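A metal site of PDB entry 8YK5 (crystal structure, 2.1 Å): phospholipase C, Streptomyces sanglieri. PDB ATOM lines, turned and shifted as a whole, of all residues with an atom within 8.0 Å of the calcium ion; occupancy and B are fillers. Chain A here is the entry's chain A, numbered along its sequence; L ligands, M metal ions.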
ATOM      1  N   MET A  13       1.035 -36.972 -23.632  1.00  0.00           N
ATOM      2  CA  MET A  13       0.576 -35.621 -23.910  1.00  0.00           C
ATOM      3  C   MET A  13      -0.554 -35.689 -24.918  1.00  0.00           C
ATOM      4  O   MET A  13      -0.369 -36.169 -26.036  1.00  0.00           O
ATOM      5  CB  MET A  13       1.696 -34.737 -24.439  1.00  0.00           C
ATOM      6  CG  MET A  13       1.260 -33.312 -24.743  1.00  0.00           C
ATOM      7  SD  MET A  13       2.647 -32.267 -25.265  1.00  0.00           S
ATOM      8  CE  MET A  13       3.223 -31.730 -23.641  1.00  0.00           C
ATOM      9  N   GLN A  14      -1.738 -35.237 -24.495  1.00  0.00           N
ATOM     10  CA  GLN A  14      -2.917 -35.084 -25.323  1.00  0.00           C
ATOM     11  C   GLN A  14      -2.933 -33.659 -25.883  1.00  0.00           C
ATOM     12  O   GLN A  14      -1.964 -32.898 -25.704  1.00  0.00           O
ATOM     13  CB  GLN A  14      -4.168 -35.429 -24.517  1.00  0.00           C
ATOM     14  CG  GLN A  14      -4.208 -36.891 -24.112  1.00  0.00           C
ATOM     15  CD  GLN A  14      -4.429 -37.805 -25.312  1.00  0.00           C
ATOM     16  OE1 GLN A  14      -3.522 -38.019 -26.133  1.00  0.00           O
ATOM     17  NE2 GLN A  14      -5.627 -38.342 -25.421  1.00  0.00           N
ATOM     18  N   GLU A  15      -4.020 -33.266 -26.555  1.00  0.00           N
ATOM     19  CA  GLU A  15      -4.016 -32.101 -27.434  1.00  0.00           C
ATOM     20  C   GLU A  15      -5.126 -31.110 -27.115  1.00  0.00           C
ATOM     21  O   GLU A  15      -6.293 -31.494 -27.021  1.00  0.00           O
ATOM     22  CB  GLU A  15      -4.159 -32.553 -28.904  1.00  0.00           C
ATOM     23  CG  GLU A  15      -2.891 -33.138 -29.506  1.00  0.00           C
ATOM     24  CD  GLU A  15      -1.894 -32.068 -29.887  1.00  0.00           C
ATOM     25  OE1 GLU A  15      -2.282 -31.241 -30.730  1.00  0.00           O
ATOM     26  OE2 GLU A  15      -0.751 -32.045 -29.353  1.00  0.00           O
ATOM     27  N   ASN A  16      -4.762 -29.827 -26.967  1.00  0.00           N
ATOM     28  CA  ASN A  16      -5.658 -28.689 -27.253  1.00  0.00           C
ATOM     29  C   ASN A  16      -6.846 -28.552 -26.288  1.00  0.00           C
ATOM     30  O   ASN A  16      -7.986 -28.413 -26.722  1.00  0.00           O
ATOM     31  CB  ASN A  16      -6.167 -28.749 -28.694  1.00  0.00           C
ATOM     32  CG  ASN A  16      -5.134 -28.303 -29.686  1.00  0.00           C
ATOM     33  OD1 ASN A  16      -4.107 -28.923 -29.814  1.00  0.00           O
ATOM     34  ND2 ASN A  16      -5.408 -27.199 -30.390  1.00  0.00           N
ATOM     35  N   ARG A  17      -6.573 -28.527 -24.984  1.00  0.00           N
ATOM     36  CA  ARG A  17      -7.612 -28.260 -24.001  1.00  0.00           C
ATOM     37  C   ARG A  17      -7.026 -27.357 -22.913  1.00  0.00           C
ATOM     38  O   ARG A  17      -5.909 -27.591 -22.463  1.00  0.00           O
ATOM     39  CB  ARG A  17      -8.151 -29.548 -23.375  1.00  0.00           C
ATOM     40  CG  ARG A  17      -8.662 -30.584 -24.380  1.00  0.00           C
ATOM     41  CD  ARG A  17      -9.941 -30.114 -25.086  1.00  0.00           C
ATOM     42  NE  ARG A  17     -10.356 -31.053 -26.130  1.00  0.00           N
ATOM     43  CZ  ARG A  17     -11.598 -31.176 -26.595  1.00  0.00           C
ATOM     44  NH1 ARG A  17     -12.575 -30.423 -26.088  1.00  0.00           N
ATOM     45  NH2 ARG A  17     -11.863 -32.064 -27.550  1.00  0.00           N
ATOM     46  N   HIS A  81      -5.468 -21.318 -32.682  1.00  0.00           N
ATOM     47  CA  HIS A  81      -4.397 -21.615 -31.752  1.00  0.00           C
ATOM     48  C   HIS A  81      -3.067 -21.180 -32.339  1.00  0.00           C
ATOM     49  O   HIS A  81      -2.073 -21.896 -32.270  1.00  0.00           O
ATOM     50  CB  HIS A  81      -4.371 -23.108 -31.401  1.00  0.00           C
ATOM     51  CG  HIS A  81      -4.551 -24.005 -32.587  1.00  0.00           C
ATOM     52  ND1 HIS A  81      -5.667 -24.779 -32.767  1.00  0.00           N
ATOM     53  CD2 HIS A  81      -3.759 -24.229 -33.661  1.00  0.00           C
ATOM     54  CE1 HIS A  81      -5.568 -25.455 -33.900  1.00  0.00           C
ATOM     55  NE2 HIS A  81      -4.412 -25.133 -34.459  1.00  0.00           N
ATOM     56  N   THR A 137       0.916 -20.603 -28.334  1.00  0.00           N
ATOM     57  CA  THR A 137       0.874 -20.816 -29.782  1.00  0.00           C
ATOM     58  C   THR A 137       0.462 -22.260 -30.021  1.00  0.00           C
ATOM     59  O   THR A 137      -0.200 -22.856 -29.157  1.00  0.00           O
ATOM     60  CB  THR A 137       2.224 -20.469 -30.432  1.00  0.00           C
ATOM     61  OG1 THR A 137       2.106 -20.596 -31.853  1.00  0.00           O
ATOM     62  CG2 THR A 137       3.340 -21.367 -29.929  1.00  0.00           C
ATOM     63  N   SER A 138       0.829 -22.841 -31.160  1.00  0.00           N
ATOM     64  CA  SER A 138       0.244 -24.096 -31.638  1.00  0.00           C
ATOM     65  C   SER A 138       1.053 -25.305 -31.131  1.00  0.00           C
ATOM     66  O   SER A 138       1.836 -25.184 -30.197  1.00  0.00           O
ATOM     67  CB  SER A 138       0.145 -24.043 -33.171  1.00  0.00           C
ATOM     68  OG  SER A 138       1.449 -24.034 -33.745  1.00  0.00           O
ATOM     69  N   THR A 139       0.870 -26.482 -31.767  1.00  0.00           N
ATOM     70  CA  THR A 139       1.378 -27.748 -31.227  1.00  0.00           C
ATOM     71  C   THR A 139       2.883 -27.846 -31.293  1.00  0.00           C
ATOM     72  O   THR A 139       3.538 -28.195 -30.311  1.00  0.00           O
ATOM     73  CB  THR A 139       0.805 -28.936 -32.003  1.00  0.00           C
ATOM     74  OG1 THR A 139      -0.606 -28.924 -31.860  1.00  0.00           O
ATOM     75  CG2 THR A 139       1.282 -30.240 -31.458  1.00  0.00           C
ATOM     76  N   SER A 140       3.448 -27.621 -32.476  1.00  0.00           N
ATOM     77  CA  SER A 140       4.855 -27.941 -32.676  1.00  0.00           C
ATOM     78  C   SER A 140       5.782 -27.191 -31.720  1.00  0.00           C
ATOM     79  O   SER A 140       6.692 -27.836 -31.175  1.00  0.00           O
ATOM     80  CB  SER A 140       5.231 -27.694 -34.133  1.00  0.00           C
ATOM     81  OG  SER A 140       6.549 -28.169 -34.365  1.00  0.00           O
ATOM     82  N   ASN A 142       5.178 -26.108 -28.724  1.00  0.00           N
ATOM     83  CA  ASN A 142       4.953 -26.665 -27.393  1.00  0.00           C
ATOM     84  C   ASN A 142       5.565 -28.043 -27.274  1.00  0.00           C
ATOM     85  O   ASN A 142       6.270 -28.331 -26.313  1.00  0.00           O
ATOM     86  CB  ASN A 142       3.465 -26.668 -27.097  1.00  0.00           C
ATOM     87  CG  ASN A 142       3.021 -25.357 -26.518  1.00  0.00           C
ATOM     88  OD1 ASN A 142       3.372 -25.045 -25.381  1.00  0.00           O
ATOM     89  ND2 ASN A 142       2.312 -24.554 -27.313  1.00  0.00           N
ATOM     90  N   ARG A 143       5.326 -28.911 -28.267  1.00  0.00           N
ATOM     91  CA  ARG A 143       5.938 -30.232 -28.229  1.00  0.00           C
ATOM     92  C   ARG A 143       7.457 -30.167 -28.295  1.00  0.00           C
ATOM     93  O   ARG A 143       8.141 -31.001 -27.698  1.00  0.00           O
ATOM     94  CB  ARG A 143       5.352 -31.102 -29.344  1.00  0.00           C
ATOM     95  CG  ARG A 143       3.950 -31.572 -28.980  1.00  0.00           C
ATOM     96  CD  ARG A 143       3.351 -32.637 -29.924  1.00  0.00           C
ATOM     97  NE  ARG A 143       2.027 -32.997 -29.431  1.00  0.00           N
ATOM     98  CZ  ARG A 143       1.744 -34.104 -28.753  1.00  0.00           C
ATOM     99  NH1 ARG A 143       2.696 -35.004 -28.517  1.00  0.00           N
ATOM    100  NH2 ARG A 143       0.516 -34.312 -28.316  1.00  0.00           N
ATOM    101  N   ASN A 163       3.932 -24.191 -36.908  1.00  0.00           N
ATOM    102  CA  ASN A 163       4.029 -25.592 -37.292  1.00  0.00           C
ATOM    103  C   ASN A 163       4.793 -25.808 -38.598  1.00  0.00           C
ATOM    104  O   ASN A 163       4.512 -26.736 -39.349  1.00  0.00           O
ATOM    105  CB  ASN A 163       2.620 -26.187 -37.370  1.00  0.00           C
ATOM    106  CG  ASN A 163       1.927 -26.220 -35.999  1.00  0.00           C
ATOM    107  OD1 ASN A 163       2.538 -25.882 -34.969  1.00  0.00           O
ATOM    108  ND2 ASN A 163       0.658 -26.618 -35.977  1.00  0.00           N
ATOM    109  N   TYR A 166       5.995 -29.261 -40.140  1.00  0.00           N
ATOM    110  CA  TYR A 166       5.105 -30.288 -40.678  1.00  0.00           C
ATOM    111  C   TYR A 166       5.242 -30.471 -42.187  1.00  0.00           C
ATOM    112  O   TYR A 166       4.729 -31.469 -42.718  1.00  0.00           O
ATOM    113  CB  TYR A 166       3.648 -29.959 -40.329  1.00  0.00           C
ATOM    114  CG  TYR A 166       3.308 -29.971 -38.851  1.00  0.00           C
ATOM    115  CD1 TYR A 166       2.056 -29.558 -38.420  1.00  0.00           C
ATOM    116  CD2 TYR A 166       4.213 -30.405 -37.889  1.00  0.00           C
ATOM    117  CE1 TYR A 166       1.717 -29.569 -37.070  1.00  0.00           C
ATOM    118  CE2 TYR A 166       3.877 -30.424 -36.533  1.00  0.00           C
ATOM    119  CZ  TYR A 166       2.628 -29.986 -36.139  1.00  0.00           C
ATOM    120  OH  TYR A 166       2.276 -29.990 -34.806  1.00  0.00           O
ATOM    121  N   PHE A 199      -0.716 -38.029 -36.350  1.00  0.00           N
ATOM    122  CA  PHE A 199      -1.203 -36.652 -36.297  1.00  0.00           C
ATOM    123  C   PHE A 199      -0.069 -35.642 -36.101  1.00  0.00           C
ATOM    124  O   PHE A 199      -0.226 -34.638 -35.413  1.00  0.00           O
ATOM    125  CB  PHE A 199      -2.269 -36.541 -35.188  1.00  0.00           C
ATOM    126  CG  PHE A 199      -3.156 -35.334 -35.288  1.00  0.00           C
ATOM    127  CD1 PHE A 199      -3.380 -34.532 -34.170  1.00  0.00           C
ATOM    128  CD2 PHE A 199      -3.790 -35.017 -36.478  1.00  0.00           C
ATOM    129  CE1 PHE A 199      -4.199 -33.420 -34.254  1.00  0.00           C
ATOM    130  CE2 PHE A 199      -4.609 -33.905 -36.563  1.00  0.00           C
ATOM    131  CZ  PHE A 199      -4.812 -33.100 -35.452  1.00  0.00           C
ATOM    132  N   ASP A 201       2.340 -35.637 -34.217  1.00  0.00           N
ATOM    133  CA  ASP A 201       2.552 -35.360 -32.804  1.00  0.00           C
ATOM    134  C   ASP A 201       3.798 -36.018 -32.229  1.00  0.00           C
ATOM    135  O   ASP A 201       4.164 -35.723 -31.085  1.00  0.00           O
ATOM    136  CB  ASP A 201       1.335 -35.765 -31.972  1.00  0.00           C
ATOM    137  CG  ASP A 201       0.202 -34.772 -32.070  1.00  0.00           C
ATOM    138  OD1 ASP A 201       0.456 -33.643 -32.515  1.00  0.00           O
ATOM    139  OD2 ASP A 201      -0.941 -35.124 -31.712  1.00  0.00           O
ATOM    140  N   SER A 302      -6.522 -38.412 -29.736  1.00  0.00           N
ATOM    141  CA  SER A 302      -5.605 -37.387 -29.247  1.00  0.00           C
ATOM    142  C   SER A 302      -6.246 -36.349 -28.343  1.00  0.00           C
ATOM    143  O   SER A 302      -5.526 -35.554 -27.736  1.00  0.00           O
ATOM    144  CB  SER A 302      -4.959 -36.657 -30.432  1.00  0.00           C
ATOM    145  OG  SER A 302      -5.898 -35.801 -31.059  1.00  0.00           O
ATOM    146  N   HIS A 304      -7.708 -33.863 -29.573  1.00  0.00           N
ATOM    147  CA  HIS A 304      -7.753 -32.646 -30.367  1.00  0.00           C
ATOM    148  C   HIS A 304      -9.181 -32.403 -30.849  1.00  0.00           C
ATOM    149  O   HIS A 304      -9.790 -33.307 -31.447  1.00  0.00           O
ATOM    150  CB  HIS A 304      -6.792 -32.741 -31.546  1.00  0.00           C
ATOM    151  CG  HIS A 304      -6.519 -31.422 -32.204  1.00  0.00           C
ATOM    152  ND1 HIS A 304      -7.469 -30.748 -32.935  1.00  0.00           N
ATOM    153  CD2 HIS A 304      -5.402 -30.649 -32.233  1.00  0.00           C
ATOM    154  CE1 HIS A 304      -6.958 -29.616 -33.387  1.00  0.00           C
ATOM    155  NE2 HIS A 304      -5.697 -29.537 -32.965  1.00  0.00           N
ATOM    156  N   PRO A 305      -9.747 -31.211 -30.628  1.00  0.00           N
ATOM    157  CA  PRO A 305     -11.158 -30.992 -30.969  1.00  0.00           C
ATOM    158  C   PRO A 305     -11.493 -31.050 -32.469  1.00  0.00           C
ATOM    159  O   PRO A 305     -12.684 -31.074 -32.820  1.00  0.00           O
ATOM    160  CB  PRO A 305     -11.443 -29.584 -30.399  1.00  0.00           C
ATOM    161  CG  PRO A 305     -10.251 -29.227 -29.562  1.00  0.00           C
ATOM    162  CD  PRO A 305      -9.098 -30.011 -30.102  1.00  0.00           C
ATOM    163  N   TYR A 340      -1.337 -31.757 -21.653  1.00  0.00           N
ATOM    164  CA  TYR A 340      -1.827 -31.263 -22.928  1.00  0.00           C
ATOM    165  C   TYR A 340      -0.794 -30.330 -23.532  1.00  0.00           C
ATOM    166  O   TYR A 340      -0.067 -29.639 -22.805  1.00  0.00           O
ATOM    167  CB  TYR A 340      -3.169 -30.525 -22.755  1.00  0.00           C
ATOM    168  CG  TYR A 340      -4.267 -31.484 -22.354  1.00  0.00           C
ATOM    169  CD1 TYR A 340      -5.160 -31.978 -23.297  1.00  0.00           C
ATOM    170  CD2 TYR A 340      -4.381 -31.936 -21.030  1.00  0.00           C
ATOM    171  CE1 TYR A 340      -6.138 -32.867 -22.946  1.00  0.00           C
ATOM    172  CE2 TYR A 340      -5.381 -32.843 -20.670  1.00  0.00           C
ATOM    173  CZ  TYR A 340      -6.245 -33.301 -21.635  1.00  0.00           C
ATOM    174  OH  TYR A 340      -7.238 -34.199 -21.317  1.00  0.00           O
ATOM    175  N   ASP A 341      -0.730 -30.287 -24.860  1.00  0.00           N
ATOM    176  CA  ASP A 341       0.333 -29.520 -25.490  1.00  0.00           C
ATOM    177  C   ASP A 341       0.082 -28.019 -25.343  1.00  0.00           C
ATOM    178  O   ASP A 341       1.020 -27.251 -25.075  1.00  0.00           O
ATOM    179  CB  ASP A 341       0.486 -29.952 -26.953  1.00  0.00           C
ATOM    180  CG  ASP A 341      -0.674 -29.517 -27.810  1.00  0.00           C
ATOM    181  OD1 ASP A 341      -1.843 -29.777 -27.430  1.00  0.00           O
ATOM    182  OD2 ASP A 341      -0.401 -28.910 -28.870  1.00  0.00           O
ATOM    183  N   GLU A 342      -1.180 -27.601 -25.430  1.00  0.00           N
ATOM    184  CA  GLU A 342      -1.580 -26.207 -25.355  1.00  0.00           C
ATOM    185  C   GLU A 342      -3.094 -26.164 -25.138  1.00  0.00           C
ATOM    186  O   GLU A 342      -3.780 -27.180 -25.214  1.00  0.00           O
ATOM    187  CB  GLU A 342      -1.232 -25.396 -26.626  1.00  0.00           C
ATOM    188  CG  GLU A 342      -1.732 -26.093 -27.815  1.00  0.00           C
ATOM    189  CD  GLU A 342      -2.836 -25.397 -28.567  1.00  0.00           C
ATOM    190  OE1 GLU A 342      -3.189 -24.222 -28.254  1.00  0.00           O
ATOM    191  OE2 GLU A 342      -3.374 -26.082 -29.499  1.00  0.00           O
ATOM    192  N   ASN A 343      -3.617 -24.954 -25.014  1.00  0.00           N
ATOM    193  CA  ASN A 343      -5.014 -24.722 -24.678  1.00  0.00           C
ATOM    194  C   ASN A 343      -5.939 -24.584 -25.883  1.00  0.00           C
ATOM    195  O   ASN A 343      -7.114 -24.235 -25.678  1.00  0.00           O
ATOM    196  CB  ASN A 343      -5.109 -23.459 -23.845  1.00  0.00           C
ATOM    197  CG  ASN A 343      -4.645 -22.230 -24.594  1.00  0.00           C
ATOM    198  OD1 ASN A 343      -3.521 -22.173 -25.114  1.00  0.00           O
ATOM    199  ND2 ASN A 343      -5.509 -21.253 -24.663  1.00  0.00           N
ATOM    200  N   ASP A 344      -5.477 -24.824 -27.119  1.00  0.00           N
ATOM    201  CA  ASP A 344      -6.258 -24.553 -28.346  1.00  0.00           C
ATOM    202  C   ASP A 344      -6.575 -23.057 -28.346  1.00  0.00           C
ATOM    203  O   ASP A 344      -5.656 -22.235 -28.134  1.00  0.00           O
ATOM    204  CB  ASP A 344      -7.467 -25.475 -28.435  1.00  0.00           C
ATOM    205  CG  ASP A 344      -8.173 -25.394 -29.789  1.00  0.00           C
ATOM    206  OD1 ASP A 344      -7.700 -26.032 -30.761  1.00  0.00           O
ATOM    207  OD2 ASP A 344      -9.196 -24.669 -29.881  1.00  0.00           O
HETATM  208  C1  LIG L   1      -3.280 -27.714 -33.319  1.00  0.00           C
HETATM  209  O1  LIG L   1      -2.972 -28.208 -32.107  1.00  0.00           O
HETATM  210  C2  LIG L   1      -2.223 -28.227 -34.221  1.00  0.00           C
HETATM  211  O2  LIG L   1      -1.082 -27.566 -33.847  1.00  0.00           O
HETATM  212  C3  LIG L   1      -2.266 -29.827 -33.972  1.00  0.00           C
HETATM  213  O3  LIG L   1      -1.261 -30.515 -34.708  1.00  0.00           O
HETATM  214 CA    CA M   1      -2.093 -29.159 -30.164  1.00  0.00          CA
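The calcium ion is bound by the side-chain amide oxygen (OD1) of Asn 16 (2.1 Å), the side-chain carboxylate (OD2) of Asp 341 (2.1 Å), the side-chain carboxylate (OE1) of Glu 15 (2.2 Å), the side-chain hydroxyl (OG1) of Thr 139 (2.3 Å), an oxygen (O1) of the ligand (2.3 Å) and the side-chain carboxylate (OD1) of Asp 341 (2.8 Å).
O of Asp 341 lies close to OD1 of Asn 142. N of Arg 17 is in hydrogen-bond range of O of Glu 342, 3.1 Å away. NE2 of His 304 is in hydrogen-bond range of ND2 of Asn 16 (3.5 Å). The side-chain carboxylate (OE1) of Glu 342 sits at hydrogen-bond distance from the backbone NH (N) of Asp 344 (2.6 Å). The backbone NH (N) of Asp 341 is in hydrogen-bond range of the backbone carbonyl oxygen (O) of Gln 14, at 3.0 Å. The side-chain amide nitrogen of Asn 16 sits at hydrogen-bond distance from the side-chain carboxylate of Glu 342, 2.5 Å away. ND2 of Asn 16 sits at hydrogen-bond distance from ND1 of His 81, 3.4 Å away. The side-chain carboxylate (OE2) of Glu 15 lies within salt-bridge range of the guanidinium group (NH2) of Arg 143 (2.8 Å).
OE2 of Glu 342 touches the calcium ion, 3.4 Å away. The nearest printed residue that does not touch the calcium ion is His 304 (4.2 Å).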
